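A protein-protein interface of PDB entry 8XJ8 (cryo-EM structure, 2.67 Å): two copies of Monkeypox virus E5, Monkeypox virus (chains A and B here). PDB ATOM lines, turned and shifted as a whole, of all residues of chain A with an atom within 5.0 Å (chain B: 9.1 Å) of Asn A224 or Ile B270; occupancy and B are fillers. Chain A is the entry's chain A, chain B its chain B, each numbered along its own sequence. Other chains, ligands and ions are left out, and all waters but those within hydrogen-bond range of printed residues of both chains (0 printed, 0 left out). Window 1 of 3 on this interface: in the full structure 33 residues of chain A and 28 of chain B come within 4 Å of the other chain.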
ATOM      1  N   VAL A 203     -16.369 -17.409  14.917  1.00  0.00           N
ATOM      2  CA  VAL A 203     -17.796 -17.670  15.058  1.00  0.00           C
ATOM      3  C   VAL A 203     -18.568 -16.935  13.968  1.00  0.00           C
ATOM      4  O   VAL A 203     -18.136 -15.898  13.452  1.00  0.00           O
ATOM      5  CB  VAL A 203     -18.317 -17.288  16.466  1.00  0.00           C
ATOM      6  CG1 VAL A 203     -18.541 -15.798  16.581  1.00  0.00           C
ATOM      7  CG2 VAL A 203     -19.588 -18.059  16.798  1.00  0.00           C
ATOM      8  N   GLU A 204     -19.713 -17.508  13.608  1.00  0.00           N
ATOM      9  CA  GLU A 204     -20.623 -16.959  12.614  1.00  0.00           C
ATOM     10  C   GLU A 204     -21.977 -16.723  13.266  1.00  0.00           C
ATOM     11  O   GLU A 204     -22.543 -17.638  13.873  1.00  0.00           O
ATOM     12  CB  GLU A 204     -20.764 -17.915  11.430  1.00  0.00           C
ATOM     13  CG  GLU A 204     -21.290 -17.282  10.163  1.00  0.00           C
ATOM     14  CD  GLU A 204     -21.175 -18.210   8.975  1.00  0.00           C
ATOM     15  OE1 GLU A 204     -20.216 -19.008   8.938  1.00  0.00           O
ATOM     16  OE2 GLU A 204     -22.043 -18.144   8.078  1.00  0.00           O
ATOM     17  N   THR A 205     -22.492 -15.506  13.143  1.00  0.00           N
ATOM     18  CA  THR A 205     -23.773 -15.139  13.733  1.00  0.00           C
ATOM     19  C   THR A 205     -24.708 -14.616  12.643  1.00  0.00           C
ATOM     20  O   THR A 205     -24.368 -14.593  11.457  1.00  0.00           O
ATOM     21  CB  THR A 205     -23.583 -14.108  14.850  1.00  0.00           C
ATOM     22  OG1 THR A 205     -22.791 -13.015  14.370  1.00  0.00           O
ATOM     23  CG2 THR A 205     -22.892 -14.741  16.046  1.00  0.00           C
ATOM     24  N   PRO A 220     -29.022 -15.859  22.194  1.00  0.00           N
ATOM     25  CA  PRO A 220     -27.841 -16.701  21.940  1.00  0.00           C
ATOM     26  C   PRO A 220     -26.937 -16.165  20.845  1.00  0.00           C
ATOM     27  O   PRO A 220     -25.723 -16.401  20.888  1.00  0.00           O
ATOM     28  CB  PRO A 220     -28.455 -18.054  21.555  1.00  0.00           C
ATOM     29  CG  PRO A 220     -29.833 -18.027  22.130  1.00  0.00           C
ATOM     30  CD  PRO A 220     -30.279 -16.605  22.027  1.00  0.00           C
ATOM     31  N   PHE A 221     -27.491 -15.448  19.864  1.00  0.00           N
ATOM     32  CA  PHE A 221     -26.673 -14.903  18.786  1.00  0.00           C
ATOM     33  C   PHE A 221     -25.650 -13.902  19.305  1.00  0.00           C
ATOM     34  O   PHE A 221     -24.584 -13.735  18.704  1.00  0.00           O
ATOM     35  CB  PHE A 221     -27.570 -14.256  17.730  1.00  0.00           C
ATOM     36  CG  PHE A 221     -28.622 -15.180  17.183  1.00  0.00           C
ATOM     37  CD1 PHE A 221     -28.311 -16.103  16.199  1.00  0.00           C
ATOM     38  CD2 PHE A 221     -29.921 -15.130  17.659  1.00  0.00           C
ATOM     39  CE1 PHE A 221     -29.276 -16.955  15.698  1.00  0.00           C
ATOM     40  CE2 PHE A 221     -30.889 -15.979  17.160  1.00  0.00           C
ATOM     41  CZ  PHE A 221     -30.566 -16.893  16.179  1.00  0.00           C
ATOM     42  N   ILE A 222     -25.952 -13.228  20.410  1.00  0.00           N
ATOM     43  CA  ILE A 222     -24.985 -12.348  21.058  1.00  0.00           C
ATOM     44  C   ILE A 222     -24.156 -13.105  22.088  1.00  0.00           C
ATOM     45  O   ILE A 222     -22.942 -12.907  22.183  1.00  0.00           O
ATOM     46  CB  ILE A 222     -25.714 -11.145  21.691  1.00  0.00           C
ATOM     47  CG1 ILE A 222     -26.051 -10.101  20.625  1.00  0.00           C
ATOM     48  CG2 ILE A 222     -24.879 -10.523  22.800  1.00  0.00           C
ATOM     49  CD1 ILE A 222     -24.848  -9.352  20.105  1.00  0.00           C
ATOM     50  N   ALA A 223     -24.794 -13.993  22.853  1.00  0.00           N
ATOM     51  CA  ALA A 223     -24.098 -14.691  23.929  1.00  0.00           C
ATOM     52  C   ALA A 223     -23.009 -15.618  23.405  1.00  0.00           C
ATOM     53  O   ALA A 223     -22.060 -15.930  24.134  1.00  0.00           O
ATOM     54  CB  ALA A 223     -25.099 -15.476  24.774  1.00  0.00           C
ATOM     55  N   ASN A 224     -23.119 -16.066  22.157  1.00  0.00           N
ATOM     56  CA  ASN A 224     -22.132 -16.973  21.588  1.00  0.00           C
ATOM     57  C   ASN A 224     -20.881 -16.257  21.093  1.00  0.00           C
ATOM     58  O   ASN A 224     -19.969 -16.915  20.586  1.00  0.00           O
ATOM     59  CB  ASN A 224     -22.754 -17.781  20.446  1.00  0.00           C
ATOM     60  CG  ASN A 224     -23.596 -18.939  20.943  1.00  0.00           C
ATOM     61  OD1 ASN A 224     -23.634 -19.224  22.140  1.00  0.00           O
ATOM     62  ND2 ASN A 224     -24.271 -19.617  20.025  1.00  0.00           N
ATOM     63  N   MET A 225     -20.817 -14.935  21.230  1.00  0.00           N
ATOM     64  CA  MET A 225     -19.662 -14.151  20.817  1.00  0.00           C
ATOM     65  C   MET A 225     -18.692 -13.880  21.959  1.00  0.00           C
ATOM     66  O   MET A 225     -17.728 -13.133  21.768  1.00  0.00           O
ATOM     67  CB  MET A 225     -20.117 -12.820  20.210  1.00  0.00           C
ATOM     68  CG  MET A 225     -21.177 -12.955  19.129  1.00  0.00           C
ATOM     69  SD  MET A 225     -21.736 -11.374  18.459  1.00  0.00           S
ATOM     70  CE  MET A 225     -20.732 -10.215  19.389  1.00  0.00           C
ATOM     71  N   HIS A 226     -18.924 -14.460  23.132  1.00  0.00           N
ATOM     72  CA  HIS A 226     -18.107 -14.173  24.305  1.00  0.00           C
ATOM     73  C   HIS A 226     -16.693 -14.710  24.113  1.00  0.00           C
ATOM     74  O   HIS A 226     -16.502 -15.903  23.857  1.00  0.00           O
ATOM     75  CB  HIS A 226     -18.757 -14.782  25.547  1.00  0.00           C
ATOM     76  CG  HIS A 226     -17.939 -14.642  26.794  1.00  0.00           C
ATOM     77  ND1 HIS A 226     -17.736 -13.429  27.418  1.00  0.00           N
ATOM     78  CD2 HIS A 226     -17.287 -15.562  27.542  1.00  0.00           C
ATOM     79  CE1 HIS A 226     -16.984 -13.608  28.489  1.00  0.00           C
ATOM     80  NE2 HIS A 226     -16.700 -14.893  28.588  1.00  0.00           N
ATOM     81  N   LYS A 228     -14.635 -14.387  21.747  1.00  0.00           N
ATOM     82  CA  LYS A 228     -14.297 -14.777  20.386  1.00  0.00           C
ATOM     83  C   LYS A 228     -13.498 -13.666  19.721  1.00  0.00           C
ATOM     84  O   LYS A 228     -13.775 -12.482  19.925  1.00  0.00           O
ATOM     85  CB  LYS A 228     -15.553 -15.079  19.567  1.00  0.00           C
ATOM     86  CG  LYS A 228     -16.339 -16.275  20.065  1.00  0.00           C
ATOM     87  CD  LYS A 228     -15.564 -17.561  19.866  1.00  0.00           C
ATOM     88  CE  LYS A 228     -16.295 -18.740  20.477  1.00  0.00           C
ATOM     89  NZ  LYS A 228     -17.558 -19.038  19.753  1.00  0.00           N
ATOM     90  N   ARG B  22     -20.660 -30.546  19.198  1.00  0.00           N
ATOM     91  CA  ARG B  22     -21.866 -29.855  19.636  1.00  0.00           C
ATOM     92  C   ARG B  22     -22.251 -30.198  21.068  1.00  0.00           C
ATOM     93  O   ARG B  22     -23.395 -29.946  21.464  1.00  0.00           O
ATOM     94  CB  ARG B  22     -23.027 -30.172  18.689  1.00  0.00           C
ATOM     95  CG  ARG B  22     -22.878 -29.558  17.304  1.00  0.00           C
ATOM     96  CD  ARG B  22     -23.871 -30.143  16.312  1.00  0.00           C
ATOM     97  NE  ARG B  22     -25.247 -29.757  16.597  1.00  0.00           N
ATOM     98  CZ  ARG B  22     -25.861 -28.711  16.059  1.00  0.00           C
ATOM     99  NH1 ARG B  22     -25.242 -27.904  15.214  1.00  0.00           N
ATOM    100  NH2 ARG B  22     -27.130 -28.472  16.374  1.00  0.00           N
ATOM    101  N   LEU B 214     -34.400 -15.696   8.904  1.00  0.00           N
ATOM    102  CA  LEU B 214     -34.077 -17.037   9.364  1.00  0.00           C
ATOM    103  C   LEU B 214     -33.545 -17.095  10.788  1.00  0.00           C
ATOM    104  O   LEU B 214     -33.476 -18.191  11.355  1.00  0.00           O
ATOM    105  CB  LEU B 214     -33.051 -17.686   8.422  1.00  0.00           C
ATOM    106  CG  LEU B 214     -33.481 -17.872   6.965  1.00  0.00           C
ATOM    107  CD1 LEU B 214     -32.309 -18.335   6.112  1.00  0.00           C
ATOM    108  CD2 LEU B 214     -34.639 -18.849   6.865  1.00  0.00           C
ATOM    109  N   ASP B 215     -33.176 -15.961  11.388  1.00  0.00           N
ATOM    110  CA  ASP B 215     -32.518 -15.981  12.690  1.00  0.00           C
ATOM    111  C   ASP B 215     -33.127 -14.991  13.677  1.00  0.00           C
ATOM    112  O   ASP B 215     -32.449 -14.569  14.619  1.00  0.00           O
ATOM    113  CB  ASP B 215     -31.016 -15.728  12.530  1.00  0.00           C
ATOM    114  CG  ASP B 215     -30.701 -14.293  12.164  1.00  0.00           C
ATOM    115  OD1 ASP B 215     -30.852 -13.931  10.978  1.00  0.00           O
ATOM    116  OD2 ASP B 215     -30.304 -13.526  13.063  1.00  0.00           O
ATOM    117  N   GLY B 217     -35.422 -14.979  16.550  1.00  0.00           N
ATOM    118  CA  GLY B 217     -36.083 -15.879  17.464  1.00  0.00           C
ATOM    119  C   GLY B 217     -35.921 -17.323  17.039  1.00  0.00           C
ATOM    120  O   GLY B 217     -35.227 -17.632  16.066  1.00  0.00           O
ATOM    121  N   PRO B 218     -36.550 -18.241  17.770  1.00  0.00           N
ATOM    122  CA  PRO B 218     -36.497 -19.653  17.378  1.00  0.00           C
ATOM    123  C   PRO B 218     -37.190 -19.887  16.045  1.00  0.00           C
ATOM    124  O   PRO B 218     -38.178 -19.233  15.705  1.00  0.00           O
ATOM    125  CB  PRO B 218     -37.227 -20.365  18.523  1.00  0.00           C
ATOM    126  CG  PRO B 218     -38.104 -19.315  19.119  1.00  0.00           C
ATOM    127  CD  PRO B 218     -37.326 -18.040  19.004  1.00  0.00           C
ATOM    128  N   ILE B 222     -36.021 -24.028   9.942  1.00  0.00           N
ATOM    129  CA  ILE B 222     -34.681 -23.971   9.368  1.00  0.00           C
ATOM    130  C   ILE B 222     -33.737 -24.810  10.219  1.00  0.00           C
ATOM    131  O   ILE B 222     -32.710 -25.295   9.733  1.00  0.00           O
ATOM    132  CB  ILE B 222     -34.186 -22.516   9.239  1.00  0.00           C
ATOM    133  CG1 ILE B 222     -33.032 -22.430   8.239  1.00  0.00           C
ATOM    134  CG2 ILE B 222     -33.770 -21.954  10.589  1.00  0.00           C
ATOM    135  CD1 ILE B 222     -33.474 -22.460   6.795  1.00  0.00           C
ATOM    136  N   ALA B 223     -34.085 -24.997  11.493  1.00  0.00           N
ATOM    137  CA  ALA B 223     -33.247 -25.774  12.393  1.00  0.00           C
ATOM    138  C   ALA B 223     -33.395 -27.275  12.192  1.00  0.00           C
ATOM    139  O   ALA B 223     -32.519 -28.032  12.624  1.00  0.00           O
ATOM    140  CB  ALA B 223     -33.564 -25.413  13.844  1.00  0.00           C
ATOM    141  N   HIS B 226     -30.702 -29.643   9.713  1.00  0.00           N
ATOM    142  CA  HIS B 226     -29.328 -29.948  10.091  1.00  0.00           C
ATOM    143  C   HIS B 226     -28.955 -31.359   9.645  1.00  0.00           C
ATOM    144  O   HIS B 226     -29.632 -32.329  10.001  1.00  0.00           O
ATOM    145  CB  HIS B 226     -29.162 -29.794  11.602  1.00  0.00           C
ATOM    146  CG  HIS B 226     -27.817 -30.202  12.115  1.00  0.00           C
ATOM    147  ND1 HIS B 226     -26.676 -29.468  11.878  1.00  0.00           N
ATOM    148  CD2 HIS B 226     -27.433 -31.263  12.864  1.00  0.00           C
ATOM    149  CE1 HIS B 226     -25.645 -30.062  12.452  1.00  0.00           C
ATOM    150  NE2 HIS B 226     -26.078 -31.153  13.058  1.00  0.00           N
ATOM    151  N   CYS B 259     -22.787 -23.289   6.344  1.00  0.00           N
ATOM    152  CA  CYS B 259     -23.399 -23.144   7.656  1.00  0.00           C
ATOM    153  C   CYS B 259     -24.598 -22.216   7.548  1.00  0.00           C
ATOM    154  O   CYS B 259     -24.523 -21.176   6.888  1.00  0.00           O
ATOM    155  CB  CYS B 259     -22.395 -22.599   8.676  1.00  0.00           C
ATOM    156  SG  CYS B 259     -23.046 -22.423  10.348  1.00  0.00           S
ATOM    157  N   VAL B 260     -25.699 -22.594   8.192  1.00  0.00           N
ATOM    158  CA  VAL B 260     -26.926 -21.809   8.203  1.00  0.00           C
ATOM    159  C   VAL B 260     -27.216 -21.401   9.640  1.00  0.00           C
ATOM    160  O   VAL B 260     -27.163 -22.236  10.550  1.00  0.00           O
ATOM    161  CB  VAL B 260     -28.108 -22.589   7.599  1.00  0.00           C
ATOM    162  CG1 VAL B 260     -29.360 -21.729   7.581  1.00  0.00           C
ATOM    163  CG2 VAL B 260     -27.766 -23.060   6.196  1.00  0.00           C
ATOM    164  N   ILE B 261     -27.509 -20.122   9.843  1.00  0.00           N
ATOM    165  CA  ILE B 261     -27.738 -19.579  11.177  1.00  0.00           C
ATOM    166  C   ILE B 261     -29.223 -19.684  11.499  1.00  0.00           C
ATOM    167  O   ILE B 261     -30.072 -19.245  10.716  1.00  0.00           O
ATOM    168  CB  ILE B 261     -27.248 -18.129  11.282  1.00  0.00           C
ATOM    169  CG1 ILE B 261     -25.787 -18.025  10.839  1.00  0.00           C
ATOM    170  CG2 ILE B 261     -27.398 -17.620  12.703  1.00  0.00           C
ATOM    171  CD1 ILE B 261     -24.861 -18.980  11.555  1.00  0.00           C
ATOM    172  N   GLY B 262     -29.534 -20.263  12.655  1.00  0.00           N
ATOM    173  CA  GLY B 262     -30.903 -20.472  13.080  1.00  0.00           C
ATOM    174  C   GLY B 262     -30.971 -21.463  14.221  1.00  0.00           C
ATOM    175  O   GLY B 262     -30.185 -22.413  14.263  1.00  0.00           O
ATOM    176  N   ARG B 263     -31.900 -21.265  15.152  1.00  0.00           N
ATOM    177  CA  ARG B 263     -31.911 -22.111  16.331  1.00  0.00           C
ATOM    178  C   ARG B 263     -33.295 -22.699  16.578  1.00  0.00           C
ATOM    179  O   ARG B 263     -34.307 -22.110  16.189  1.00  0.00           O
ATOM    180  CB  ARG B 263     -31.462 -21.327  17.572  1.00  0.00           C
ATOM    181  CG  ARG B 263     -32.419 -20.237  18.013  1.00  0.00           C
ATOM    182  CD  ARG B 263     -31.906 -19.551  19.265  1.00  0.00           C
ATOM    183  NE  ARG B 263     -32.830 -18.538  19.756  1.00  0.00           N
ATOM    184  CZ  ARG B 263     -33.802 -18.769  20.627  1.00  0.00           C
ATOM    185  NH1 ARG B 263     -34.015 -19.979  21.119  1.00  0.00           N
ATOM    186  NH2 ARG B 263     -34.577 -17.763  21.018  1.00  0.00           N
ATOM    187  N   PRO B 264     -33.365 -23.873  17.209  1.00  0.00           N
ATOM    188  CA  PRO B 264     -34.667 -24.445  17.574  1.00  0.00           C
ATOM    189  C   PRO B 264     -35.265 -23.776  18.799  1.00  0.00           C
ATOM    190  O   PRO B 264     -34.707 -22.808  19.325  1.00  0.00           O
ATOM    191  CB  PRO B 264     -34.339 -25.919  17.858  1.00  0.00           C
ATOM    192  CG  PRO B 264     -32.974 -26.145  17.284  1.00  0.00           C
ATOM    193  CD  PRO B 264     -32.272 -24.836  17.409  1.00  0.00           C
ATOM    194  N   SER B 267     -33.268 -23.798  22.696  1.00  0.00           N
ATOM    195  CA  SER B 267     -31.948 -24.248  22.280  1.00  0.00           C
ATOM    196  C   SER B 267     -31.008 -23.060  22.131  1.00  0.00           C
ATOM    197  O   SER B 267     -31.416 -21.969  21.727  1.00  0.00           O
ATOM    198  CB  SER B 267     -32.015 -25.027  20.961  1.00  0.00           C
ATOM    199  OG  SER B 267     -30.728 -25.448  20.547  1.00  0.00           O
ATOM    200  N   ASN B 268     -29.739 -23.293  22.463  1.00  0.00           N
ATOM    201  CA  ASN B 268     -28.686 -22.295  22.333  1.00  0.00           C
ATOM    202  C   ASN B 268     -27.813 -22.507  21.103  1.00  0.00           C
ATOM    203  O   ASN B 268     -26.886 -21.724  20.878  1.00  0.00           O
ATOM    204  CB  ASN B 268     -27.804 -22.293  23.586  1.00  0.00           C
ATOM    205  CG  ASN B 268     -28.402 -21.486  24.720  1.00  0.00           C
ATOM    206  OD1 ASN B 268     -28.714 -20.307  24.561  1.00  0.00           O
ATOM    207  ND2 ASN B 268     -28.559 -22.119  25.875  1.00  0.00           N
ATOM    208  N   LYS B 269     -28.082 -23.539  20.307  1.00  0.00           N
ATOM    209  CA  LYS B 269     -27.271 -23.859  19.140  1.00  0.00           C
ATOM    210  C   LYS B 269     -27.804 -23.093  17.935  1.00  0.00           C
ATOM    211  O   LYS B 269     -28.963 -23.268  17.547  1.00  0.00           O
ATOM    212  CB  LYS B 269     -27.287 -25.362  18.873  1.00  0.00           C
ATOM    213  CG  LYS B 269     -26.310 -26.152  19.725  1.00  0.00           C
ATOM    214  CD  LYS B 269     -26.551 -27.645  19.589  1.00  0.00           C
ATOM    215  CE  LYS B 269     -26.862 -28.277  20.936  1.00  0.00           C
ATOM    216  NZ  LYS B 269     -27.034 -29.752  20.829  1.00  0.00           N
ATOM    217  N   ILE B 270     -26.955 -22.259  17.338  1.00  0.00           N
ATOM    218  CA  ILE B 270     -27.371 -21.348  16.279  1.00  0.00           C
ATOM    219  C   ILE B 270     -26.751 -21.683  14.935  1.00  0.00           C
ATOM    220  O   ILE B 270     -26.969 -20.940  13.968  1.00  0.00           O
ATOM    221  CB  ILE B 270     -27.070 -19.884  16.653  1.00  0.00           C
ATOM    222  CG1 ILE B 270     -25.575 -19.694  16.910  1.00  0.00           C
ATOM    223  CG2 ILE B 270     -27.878 -19.468  17.871  1.00  0.00           C
ATOM    224  CD1 ILE B 270     -25.092 -18.281  16.683  1.00  0.00           C
ATOM    225  N   ASN B 271     -25.987 -22.766  14.833  1.00  0.00           N
ATOM    226  CA  ASN B 271     -25.326 -23.143  13.590  1.00  0.00           C
ATOM    227  C   ASN B 271     -25.809 -24.515  13.142  1.00  0.00           C
ATOM    228  O   ASN B 271     -25.867 -25.451  13.946  1.00  0.00           O
ATOM    229  CB  ASN B 271     -23.803 -23.138  13.754  1.00  0.00           C
ATOM    230  CG  ASN B 271     -23.333 -24.013  14.897  1.00  0.00           C
ATOM    231  OD1 ASN B 271     -24.080 -24.283  15.836  1.00  0.00           O
ATOM    232  ND2 ASN B 271     -22.086 -24.462  14.822  1.00  0.00           N
ATOM    233  N   ASN B 272     -26.156 -24.630  11.860  1.00  0.00           N
ATOM    234  CA  ASN B 272     -26.604 -25.883  11.270  1.00  0.00           C
ATOM    235  C   ASN B 272     -25.743 -26.185  10.055  1.00  0.00           C
ATOM    236  O   ASN B 272     -25.519 -25.303   9.220  1.00  0.00           O
ATOM    237  CB  ASN B 272     -28.079 -25.808  10.865  1.00  0.00           C
ATOM    238  CG  ASN B 272     -28.959 -25.248  11.964  1.00  0.00           C
ATOM    239  OD1 ASN B 272     -28.931 -25.719  13.100  1.00  0.00           O
ATOM    240  ND2 ASN B 272     -29.740 -24.229  11.632  1.00  0.00           N
ATOM    241  N   ARG B 273     -25.266 -27.423   9.952  1.00  0.00           N
ATOM    242  CA  ARG B 273     -24.440 -27.818   8.819  1.00  0.00           C
ATOM    243  C   ARG B 273     -25.324 -28.186   7.634  1.00  0.00           C
ATOM    244  O   ARG B 273     -26.262 -28.977   7.768  1.00  0.00           O
ATOM    245  CB  ARG B 273     -23.531 -28.987   9.195  1.00  0.00           C
ATOM    246  CG  ARG B 273     -22.145 -28.893   8.578  1.00  0.00           C
ATOM    247  CD  ARG B 273     -21.377 -30.194   8.704  1.00  0.00           C
ATOM    248  NE  ARG B 273     -21.428 -30.739  10.054  1.00  0.00           N
ATOM    249  CZ  ARG B 273     -20.863 -31.881  10.420  1.00  0.00           C
ATOM    250  NH1 ARG B 273     -20.195 -32.629   9.557  1.00  0.00           N
ATOM    251  NH2 ARG B 273     -20.973 -32.284  11.683  1.00  0.00           N
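Among the printed residues, pairs that only touch across the chains: Glu A204 with Ile B261, Glu A204 with Ile B270, Thr A205 with Ile B261, Pro A220 with Arg B263, Pro A220 with Asn B268, Pro A220 with Ile B270, Phe A221 with Asp B215, Phe A221 with Ile B261, Phe A221 with Ile B270 and Asn A224 with Ile B270.
O of Asn B268 is in hydrogen-bond range of ND2 of Asn A224 (3.5 Å).
Of the printed residues of chain B, Thr A205 touches Ile B261 (3.8 Å).
Phe A221 touches just these residues of chain B: Asp B215, Ile B261 and Ile B270.
Of chain B, only Asn B268 and Ile B270 come within 4 Å of Asn A224.
Of the printed residues of chain A, Asn B268 touches Pro A220 and Asn A224.
Of the printed residues of chain A, Ile B270 touches Glu A204, Pro A220, Phe A221 and Asn A224.
Printed residues of chain A that touch a printed residue of chain B: Glu A204, Thr A205, Pro A220, Phe A221 and Asn A224.
Hydrophobic or aromatic side chains of chain A within 4 Å of the printed part of chain B: Pro A220 and Phe A221.
Among the printed residues, no Asp or Glu carboxylate lies within 4 Å of a Lys or Arg side-chain nitrogen of the other chain.
3 positions are printed for both chains.
The side-chain amino group (NZ) of Lys A228 lies within hydrogen-bond range of the backbone carbonyl oxygen (O) of Asn A224 (3.3 Å).
N of Gly B262 sits at hydrogen-bond distance from O of Ile B270, at 3.0 Å.
The guanidinium group (NH1) of Arg B263 sits at hydrogen-bond distance from the backbone carbonyl oxygen (O) of Ser B267.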
